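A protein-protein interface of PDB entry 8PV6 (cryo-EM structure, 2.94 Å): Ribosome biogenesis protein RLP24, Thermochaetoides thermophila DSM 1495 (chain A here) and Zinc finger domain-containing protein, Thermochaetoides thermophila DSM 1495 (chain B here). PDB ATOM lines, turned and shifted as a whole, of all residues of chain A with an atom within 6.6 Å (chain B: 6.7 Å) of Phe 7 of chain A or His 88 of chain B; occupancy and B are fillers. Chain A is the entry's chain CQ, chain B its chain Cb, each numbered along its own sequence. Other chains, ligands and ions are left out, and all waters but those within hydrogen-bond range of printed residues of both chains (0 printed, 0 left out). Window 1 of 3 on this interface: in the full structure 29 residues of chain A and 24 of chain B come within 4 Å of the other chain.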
ATOM      1  N   ASN A   5      10.001  16.152   2.623  1.00  0.00           N
ATOM      2  CA  ASN A   5       9.050  16.204   3.720  1.00  0.00           C
ATOM      3  C   ASN A   5       9.648  15.501   4.926  1.00  0.00           C
ATOM      4  O   ASN A   5      10.411  14.542   4.786  1.00  0.00           O
ATOM      5  CB  ASN A   5       7.717  15.567   3.332  1.00  0.00           C
ATOM      6  CG  ASN A   5       6.835  16.511   2.544  1.00  0.00           C
ATOM      7  OD1 ASN A   5       6.336  17.502   3.074  1.00  0.00           O
ATOM      8  ND2 ASN A   5       6.652  16.217   1.261  1.00  0.00           N
ATOM      9  N   CYS A   6       9.311  16.000   6.112  1.00  0.00           N
ATOM     10  CA  CYS A   6       9.799  15.395   7.338  1.00  0.00           C
ATOM     11  C   CYS A   6       9.195  14.009   7.510  1.00  0.00           C
ATOM     12  O   CYS A   6       8.001  13.801   7.284  1.00  0.00           O
ATOM     13  CB  CYS A   6       9.458  16.277   8.537  1.00  0.00           C
ATOM     14  SG  CYS A   6      10.054  15.665  10.124  1.00  0.00           S
ATOM     15  N   PHE A   7      10.046  13.051   7.879  1.00  0.00           N
ATOM     16  CA  PHE A   7       9.570  11.698   8.139  1.00  0.00           C
ATOM     17  C   PHE A   7       8.638  11.670   9.340  1.00  0.00           C
ATOM     18  O   PHE A   7       7.634  10.950   9.340  1.00  0.00           O
ATOM     19  CB  PHE A   7      10.762  10.767   8.358  1.00  0.00           C
ATOM     20  CG  PHE A   7      10.381   9.394   8.823  1.00  0.00           C
ATOM     21  CD1 PHE A   7       9.791   8.492   7.955  1.00  0.00           C
ATOM     22  CD2 PHE A   7      10.615   9.004  10.131  1.00  0.00           C
ATOM     23  CE1 PHE A   7       9.442   7.229   8.382  1.00  0.00           C
ATOM     24  CE2 PHE A   7      10.265   7.745  10.563  1.00  0.00           C
ATOM     25  CZ  PHE A   7       9.680   6.855   9.685  1.00  0.00           C
ATOM     26  N   PHE A   8       8.940  12.466  10.360  1.00  0.00           N
ATOM     27  CA  PHE A   8       8.206  12.413  11.616  1.00  0.00           C
ATOM     28  C   PHE A   8       6.889  13.175  11.538  1.00  0.00           C
ATOM     29  O   PHE A   8       5.816  12.584  11.699  1.00  0.00           O
ATOM     30  CB  PHE A   8       9.071  12.972  12.744  1.00  0.00           C
ATOM     31  CG  PHE A   8       8.656  12.514  14.106  1.00  0.00           C
ATOM     32  CD1 PHE A   8       9.199  11.367  14.657  1.00  0.00           C
ATOM     33  CD2 PHE A   8       7.718  13.225  14.834  1.00  0.00           C
ATOM     34  CE1 PHE A   8       8.820  10.942  15.910  1.00  0.00           C
ATOM     35  CE2 PHE A   8       7.332  12.801  16.085  1.00  0.00           C
ATOM     36  CZ  PHE A   8       7.880  11.656  16.621  1.00  0.00           C
ATOM     37  N   CYS A   9       6.953  14.483  11.288  1.00  0.00           N
ATOM     38  CA  CYS A   9       5.757  15.310  11.390  1.00  0.00           C
ATOM     39  C   CYS A   9       5.190  15.713  10.035  1.00  0.00           C
ATOM     40  O   CYS A   9       4.086  16.263   9.984  1.00  0.00           O
ATOM     41  CB  CYS A   9       6.058  16.558  12.216  1.00  0.00           C
ATOM     42  SG  CYS A   9       7.108  17.754  11.385  1.00  0.00           S
ATOM     43  N   GLY A  10       5.912  15.468   8.947  1.00  0.00           N
ATOM     44  CA  GLY A  10       5.384  15.761   7.630  1.00  0.00           C
ATOM     45  C   GLY A  10       5.487  17.201   7.190  1.00  0.00           C
ATOM     46  O   GLY A  10       4.952  17.551   6.134  1.00  0.00           O
ATOM     47  N   ARG A  11       6.151  18.050   7.965  1.00  0.00           N
ATOM     48  CA  ARG A  11       6.342  19.442   7.596  1.00  0.00           C
ATOM     49  C   ARG A  11       7.354  19.509   6.459  1.00  0.00           C
ATOM     50  O   ARG A  11       8.263  18.679   6.384  1.00  0.00           O
ATOM     51  CB  ARG A  11       6.779  20.230   8.833  1.00  0.00           C
ATOM     52  CG  ARG A  11       6.712  21.738   8.720  1.00  0.00           C
ATOM     53  CD  ARG A  11       7.109  22.451   9.999  1.00  0.00           C
ATOM     54  NE  ARG A  11       8.534  22.340  10.282  1.00  0.00           N
ATOM     55  CZ  ARG A  11       9.118  22.826  11.367  1.00  0.00           C
ATOM     56  NH1 ARG A  11       8.428  23.475  12.288  1.00  0.00           N
ATOM     57  NH2 ARG A  11      10.429  22.674  11.520  1.00  0.00           N
ATOM     58  N   ARG A  23      20.102   4.546   8.261  1.00  0.00           N
ATOM     59  CA  ARG A  23      20.076   3.260   8.934  1.00  0.00           C
ATOM     60  C   ARG A  23      20.805   2.218   8.097  1.00  0.00           C
ATOM     61  O   ARG A  23      20.899   2.332   6.873  1.00  0.00           O
ATOM     62  CB  ARG A  23      18.635   2.823   9.187  1.00  0.00           C
ATOM     63  CG  ARG A  23      18.439   1.959  10.413  1.00  0.00           C
ATOM     64  CD  ARG A  23      16.994   2.006  10.855  1.00  0.00           C
ATOM     65  NE  ARG A  23      16.115   1.392   9.869  1.00  0.00           N
ATOM     66  CZ  ARG A  23      14.797   1.315   9.986  1.00  0.00           C
ATOM     67  NH1 ARG A  23      14.168   1.797  11.044  1.00  0.00           N
ATOM     68  NH2 ARG A  23      14.093   0.744   9.013  1.00  0.00           N
ATOM     69  N   LYS A  27      17.784   2.422   4.682  1.00  0.00           N
ATOM     70  CA  LYS A  27      16.768   3.458   4.780  1.00  0.00           C
ATOM     71  C   LYS A  27      17.388   4.783   5.202  1.00  0.00           C
ATOM     72  O   LYS A  27      18.398   4.813   5.912  1.00  0.00           O
ATOM     73  CB  LYS A  27      15.672   3.061   5.769  1.00  0.00           C
ATOM     74  CG  LYS A  27      14.973   1.762   5.417  1.00  0.00           C
ATOM     75  CD  LYS A  27      14.037   1.948   4.239  1.00  0.00           C
ATOM     76  CE  LYS A  27      13.501   0.615   3.750  1.00  0.00           C
ATOM     77  NZ  LYS A  27      13.356  -0.363   4.861  1.00  0.00           N
ATOM     78  N   ALA A  28      16.783   5.872   4.745  1.00  0.00           N
ATOM     79  CA  ALA A  28      17.168   7.220   5.124  1.00  0.00           C
ATOM     80  C   ALA A  28      15.960   7.954   5.689  1.00  0.00           C
ATOM     81  O   ALA A  28      14.869   7.923   5.113  1.00  0.00           O
ATOM     82  CB  ALA A  28      17.732   7.990   3.929  1.00  0.00           C
ATOM     83  N   PHE A  29      16.162   8.613   6.825  1.00  0.00           N
ATOM     84  CA  PHE A  29      15.090   9.315   7.521  1.00  0.00           C
ATOM     85  C   PHE A  29      15.454  10.788   7.588  1.00  0.00           C
ATOM     86  O   PHE A  29      16.501  11.142   8.137  1.00  0.00           O
ATOM     87  CB  PHE A  29      14.873   8.748   8.930  1.00  0.00           C
ATOM     88  CG  PHE A  29      14.569   7.273   8.959  1.00  0.00           C
ATOM     89  CD1 PHE A  29      15.587   6.332   8.942  1.00  0.00           C
ATOM     90  CD2 PHE A  29      13.260   6.828   9.005  1.00  0.00           C
ATOM     91  CE1 PHE A  29      15.303   4.984   8.965  1.00  0.00           C
ATOM     92  CE2 PHE A  29      12.973   5.481   9.031  1.00  0.00           C
ATOM     93  CZ  PHE A  29      13.994   4.558   9.010  1.00  0.00           C
ATOM     94  N   ARG A  30      14.596  11.640   7.040  1.00  0.00           N
ATOM     95  CA  ARG A  30      14.838  13.074   6.997  1.00  0.00           C
ATOM     96  C   ARG A  30      13.947  13.775   8.012  1.00  0.00           C
ATOM     97  O   ARG A  30      12.724  13.615   7.984  1.00  0.00           O
ATOM     98  CB  ARG A  30      14.581  13.628   5.595  1.00  0.00           C
ATOM     99  CG  ARG A  30      14.607  15.140   5.515  1.00  0.00           C
ATOM    100  CD  ARG A  30      16.019  15.674   5.658  1.00  0.00           C
ATOM    101  NE  ARG A  30      16.062  17.130   5.619  1.00  0.00           N
ATOM    102  CZ  ARG A  30      16.041  17.854   4.508  1.00  0.00           C
ATOM    103  NH1 ARG A  30      15.979  17.289   3.315  1.00  0.00           N
ATOM    104  NH2 ARG A  30      16.086  19.179   4.598  1.00  0.00           N
ATOM    105  N   PHE A  31      14.561  14.547   8.903  1.00  0.00           N
ATOM    106  CA  PHE A  31      13.855  15.274   9.944  1.00  0.00           C
ATOM    107  C   PHE A  31      14.044  16.765   9.726  1.00  0.00           C
ATOM    108  O   PHE A  31      15.165  17.228   9.499  1.00  0.00           O
ATOM    109  CB  PHE A  31      14.364  14.878  11.328  1.00  0.00           C
ATOM    110  CG  PHE A  31      14.361  13.404  11.560  1.00  0.00           C
ATOM    111  CD1 PHE A  31      13.177  12.734  11.803  1.00  0.00           C
ATOM    112  CD2 PHE A  31      15.540  12.683  11.515  1.00  0.00           C
ATOM    113  CE1 PHE A  31      13.173  11.377  12.007  1.00  0.00           C
ATOM    114  CE2 PHE A  31      15.538  11.325  11.720  1.00  0.00           C
ATOM    115  CZ  PHE A  31      14.354  10.674  11.961  1.00  0.00           C
ATOM    116  N   CYS A  32      12.939  17.506   9.797  1.00  0.00           N
ATOM    117  CA  CYS A  32      12.975  18.941   9.546  1.00  0.00           C
ATOM    118  C   CYS A  32      13.581  19.721  10.703  1.00  0.00           C
ATOM    119  O   CYS A  32      14.028  20.856  10.503  1.00  0.00           O
ATOM    120  CB  CYS A  32      11.567  19.455   9.252  1.00  0.00           C
ATOM    121  SG  CYS A  32      10.455  19.453  10.676  1.00  0.00           S
ATOM    122  N   PHE A  40      12.341  10.939  17.440  1.00  0.00           N
ATOM    123  CA  PHE A  40      12.669   9.682  16.772  1.00  0.00           C
ATOM    124  C   PHE A  40      13.722   8.899  17.550  1.00  0.00           C
ATOM    125  O   PHE A  40      13.611   7.678  17.705  1.00  0.00           O
ATOM    126  CB  PHE A  40      13.151   9.952  15.347  1.00  0.00           C
ATOM    127  CG  PHE A  40      13.508   8.707  14.583  1.00  0.00           C
ATOM    128  CD1 PHE A  40      12.518   7.915  14.026  1.00  0.00           C
ATOM    129  CD2 PHE A  40      14.832   8.330  14.416  1.00  0.00           C
ATOM    130  CE1 PHE A  40      12.841   6.773  13.321  1.00  0.00           C
ATOM    131  CE2 PHE A  40      15.160   7.191  13.712  1.00  0.00           C
ATOM    132  CZ  PHE A  40      14.163   6.411  13.165  1.00  0.00           C
ATOM    133  N   PRO A  46       5.085   8.855  15.864  1.00  0.00           N
ATOM    134  CA  PRO A  46       4.423  10.033  15.279  1.00  0.00           C
ATOM    135  C   PRO A  46       2.915   9.900  15.189  1.00  0.00           C
ATOM    136  O   PRO A  46       2.214  10.919  15.151  1.00  0.00           O
ATOM    137  CB  PRO A  46       5.058  10.139  13.886  1.00  0.00           C
ATOM    138  CG  PRO A  46       6.307   9.343  13.960  1.00  0.00           C
ATOM    139  CD  PRO A  46       6.053   8.248  14.937  1.00  0.00           C
ATOM    140  N   ALA A  54       0.773  12.566  10.766  1.00  0.00           N
ATOM    141  CA  ALA A  54       0.446  11.153  10.932  1.00  0.00           C
ATOM    142  C   ALA A  54      -0.740  10.968  11.868  1.00  0.00           C
ATOM    143  O   ALA A  54      -1.679  10.222  11.558  1.00  0.00           O
ATOM    144  CB  ALA A  54       1.663  10.400  11.459  1.00  0.00           C
ATOM    145  N   ASP B  20       9.962  -1.053  13.009  1.00  0.00           N
ATOM    146  CA  ASP B  20       9.778  -1.457  11.618  1.00  0.00           C
ATOM    147  C   ASP B  20      10.750  -2.565  11.223  1.00  0.00           C
ATOM    148  O   ASP B  20      10.381  -3.497  10.495  1.00  0.00           O
ATOM    149  CB  ASP B  20       9.884  -0.235  10.699  1.00  0.00           C
ATOM    150  CG  ASP B  20      11.250   0.446  10.744  1.00  0.00           C
ATOM    151  OD1 ASP B  20      12.141   0.026  11.514  1.00  0.00           O
ATOM    152  OD2 ASP B  20      11.431   1.427   9.995  1.00  0.00           O
ATOM    153  N   TYR B  86       5.575   2.671  12.383  1.00  0.00           N
ATOM    154  CA  TYR B  86       5.460   3.827  11.510  1.00  0.00           C
ATOM    155  C   TYR B  86       6.537   3.761  10.435  1.00  0.00           C
ATOM    156  O   TYR B  86       7.726   3.645  10.746  1.00  0.00           O
ATOM    157  CB  TYR B  86       5.592   5.106  12.334  1.00  0.00           C
ATOM    158  CG  TYR B  86       5.442   6.376  11.548  1.00  0.00           C
ATOM    159  CD1 TYR B  86       4.190   6.846  11.194  1.00  0.00           C
ATOM    160  CD2 TYR B  86       6.552   7.115  11.174  1.00  0.00           C
ATOM    161  CE1 TYR B  86       4.050   8.011  10.479  1.00  0.00           C
ATOM    162  CE2 TYR B  86       6.420   8.283  10.462  1.00  0.00           C
ATOM    163  CZ  TYR B  86       5.167   8.728  10.118  1.00  0.00           C
ATOM    164  OH  TYR B  86       5.033   9.897   9.410  1.00  0.00           O
ATOM    165  N   THR B  87       6.120   3.831   9.175  1.00  0.00           N
ATOM    166  CA  THR B  87       7.008   3.625   8.042  1.00  0.00           C
ATOM    167  C   THR B  87       6.918   4.785   7.060  1.00  0.00           C
ATOM    168  O   THR B  87       6.146   5.733   7.239  1.00  0.00           O
ATOM    169  CB  THR B  87       6.689   2.307   7.327  1.00  0.00           C
ATOM    170  OG1 THR B  87       5.277   2.212   7.102  1.00  0.00           O
ATOM    171  CG2 THR B  87       7.147   1.125   8.158  1.00  0.00           C
ATOM    172  N   HIS B  88       7.733   4.686   6.005  1.00  0.00           N
ATOM    173  CA  HIS B  88       7.799   5.741   4.999  1.00  0.00           C
ATOM    174  C   HIS B  88       6.516   5.829   4.188  1.00  0.00           C
ATOM    175  O   HIS B  88       6.098   6.929   3.814  1.00  0.00           O
ATOM    176  CB  HIS B  88       8.993   5.512   4.072  1.00  0.00           C
ATOM    177  CG  HIS B  88      10.311   5.872   4.681  1.00  0.00           C
ATOM    178  ND1 HIS B  88      11.172   4.929   5.199  1.00  0.00           N
ATOM    179  CD2 HIS B  88      10.916   7.070   4.861  1.00  0.00           C
ATOM    180  CE1 HIS B  88      12.251   5.528   5.667  1.00  0.00           C
ATOM    181  NE2 HIS B  88      12.120   6.829   5.476  1.00  0.00           N
ATOM    182  N   GLU B  89       5.880   4.689   3.906  1.00  0.00           N
ATOM    183  CA  GLU B  89       4.614   4.705   3.180  1.00  0.00           C
ATOM    184  C   GLU B  89       3.515   5.357   4.009  1.00  0.00           C
ATOM    185  O   GLU B  89       2.680   6.100   3.479  1.00  0.00           O
ATOM    186  CB  GLU B  89       4.213   3.284   2.778  1.00  0.00           C
ATOM    187  CG  GLU B  89       5.125   2.627   1.745  1.00  0.00           C
ATOM    188  CD  GLU B  89       6.371   2.005   2.348  1.00  0.00           C
ATOM    189  OE1 GLU B  89       6.510   2.021   3.590  1.00  0.00           O
ATOM    190  OE2 GLU B  89       7.217   1.505   1.577  1.00  0.00           O
ATOM    191  N   GLU B  90       3.513   5.106   5.320  1.00  0.00           N
ATOM    192  CA  GLU B  90       2.566   5.779   6.202  1.00  0.00           C
ATOM    193  C   GLU B  90       2.861   7.273   6.277  1.00  0.00           C
ATOM    194  O   GLU B  90       1.935   8.093   6.323  1.00  0.00           O
ATOM    195  CB  GLU B  90       2.605   5.139   7.590  1.00  0.00           C
ATOM    196  CG  GLU B  90       1.795   5.861   8.651  1.00  0.00           C
ATOM    197  CD  GLU B  90       1.186   4.911   9.658  1.00  0.00           C
ATOM    198  OE1 GLU B  90       1.427   3.691   9.546  1.00  0.00           O
ATOM    199  OE2 GLU B  90       0.468   5.382  10.564  1.00  0.00           O
ATOM    200  N   ALA B  91       4.146   7.640   6.260  1.00  0.00           N
ATOM    201  CA  ALA B  91       4.527   9.050   6.250  1.00  0.00           C
ATOM    202  C   ALA B  91       4.031   9.750   4.990  1.00  0.00           C
ATOM    203  O   ALA B  91       3.553  10.889   5.045  1.00  0.00           O
ATOM    204  CB  ALA B  91       6.046   9.177   6.371  1.00  0.00           C
ATOM    205  N   MET B  92       4.149   9.082   3.841  1.00  0.00           N
ATOM    206  CA  MET B  92       3.637   9.642   2.592  1.00  0.00           C
ATOM    207  C   MET B  92       2.115   9.724   2.596  1.00  0.00           C
ATOM    208  O   MET B  92       1.538  10.703   2.109  1.00  0.00           O
ATOM    209  CB  MET B  92       4.120   8.810   1.409  1.00  0.00           C
ATOM    210  CG  MET B  92       5.618   8.812   1.211  1.00  0.00           C
ATOM    211  SD  MET B  92       6.034   8.528  -0.514  1.00  0.00           S
ATOM    212  CE  MET B  92       5.708   6.772  -0.614  1.00  0.00           C
ATOM    213  N   ALA B  93       1.445   8.701   3.134  1.00  0.00           N
ATOM    214  CA  ALA B  93      -0.014   8.703   3.156  1.00  0.00           C
ATOM    215  C   ALA B  93      -0.556   9.754   4.116  1.00  0.00           C
ATOM    216  O   ALA B  93      -1.697  10.207   3.972  1.00  0.00           O
ATOM    217  CB  ALA B  93      -0.535   7.317   3.530  1.00  0.00           C
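The side-chain sulfur of Cys 6 of chain A sits close to the backbone NH of Phe 8 of chain A (3.4 Å).
The backbone NH (N) of Phe 7 of chain A lies within hydrogen-bond range of the backbone carbonyl oxygen (O) of Arg 30 of chain A, at 2.7 Å.
Of chain B, only Tyr 86 (2.8 Å), Thr 87 (3.8 Å), His 88 (3.6 Å) and Ala 91 (3.8 Å) come within 4 Å of Phe 7 of chain A.
Printed residues of chain B within 4 Å of Arg 23 of chain A: Asp 20 (2.7 Å).
Arg 30 of chain A touches none of the printed residues of chain B.
Of the printed residues of chain B, Pro 46 of chain A touches Tyr 86 (3.6 Å).
Of the printed residues of chain B, Ala 54 of chain A touches Tyr 86.
Printed residues of chain A within 4 Å of Tyr 86 of chain B: Phe 7, Phe 8, Pro 46 and Ala 54.
Of the printed residues of chain A, His 88 of chain B touches Phe 7, Ala 28 and Phe 29.
The nearest residue of chain B that does not touch Phe 7 of chain A is Asp 20 of chain B (5.7 Å).
The nearest residue of chain A that does not touch His 88 of chain B is Lys 27 of chain A (4.2 Å).
The nearest printed residue of chain B that does not touch Ala 54 of chain A is Glu 90 of chain B (5.2 Å).
O of Phe 7 of chain A lies within hydrogen-bond range of OH of Tyr 86 of chain B.
The side-chain carboxylate (OD1) of Asp 20 of chain B lies within salt-bridge range of the guanidinium group (NH1) of Arg 23 of chain A, at 2.7 Å.
The backbone carbonyl oxygen of Ala 28 of chain A lies within hydrogen-bond range of a ring nitrogen (NE2) of His 88 of chain B, at 3.0 Å.
Along chain B the printed residues that touch a printed residue of chain A span positions 20 to 91.
Of the 17 printed residues of chain A, 7 touch a printed residue of chain B.
Hydrophobic or aromatic side chains of chain A that line the printed part of chain B: Phe 7, Phe 29, Pro 46 and Ala 54.
Along chain A the printed residues that touch a printed residue of chain B span positions 7 to 54.
Among the printed residues, pairs that only touch across the chains: Phe 7 of chain A with Thr 87 of chain B (3.8 Å), Phe 7 of chain A with His 88 of chain B (3.6 Å), Phe 7 of chain A with Ala 91 of chain B (3.8 Å), Phe 8 of chain A with Tyr 86 of chain B (3.6 Å), Phe 29 of chain A with His 88 of chain B (3.4 Å), Pro 46 of chain A with Tyr 86 of chain B (3.6 Å) and Ala 54 of chain A with Tyr 86 of chain B (3.5 Å).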
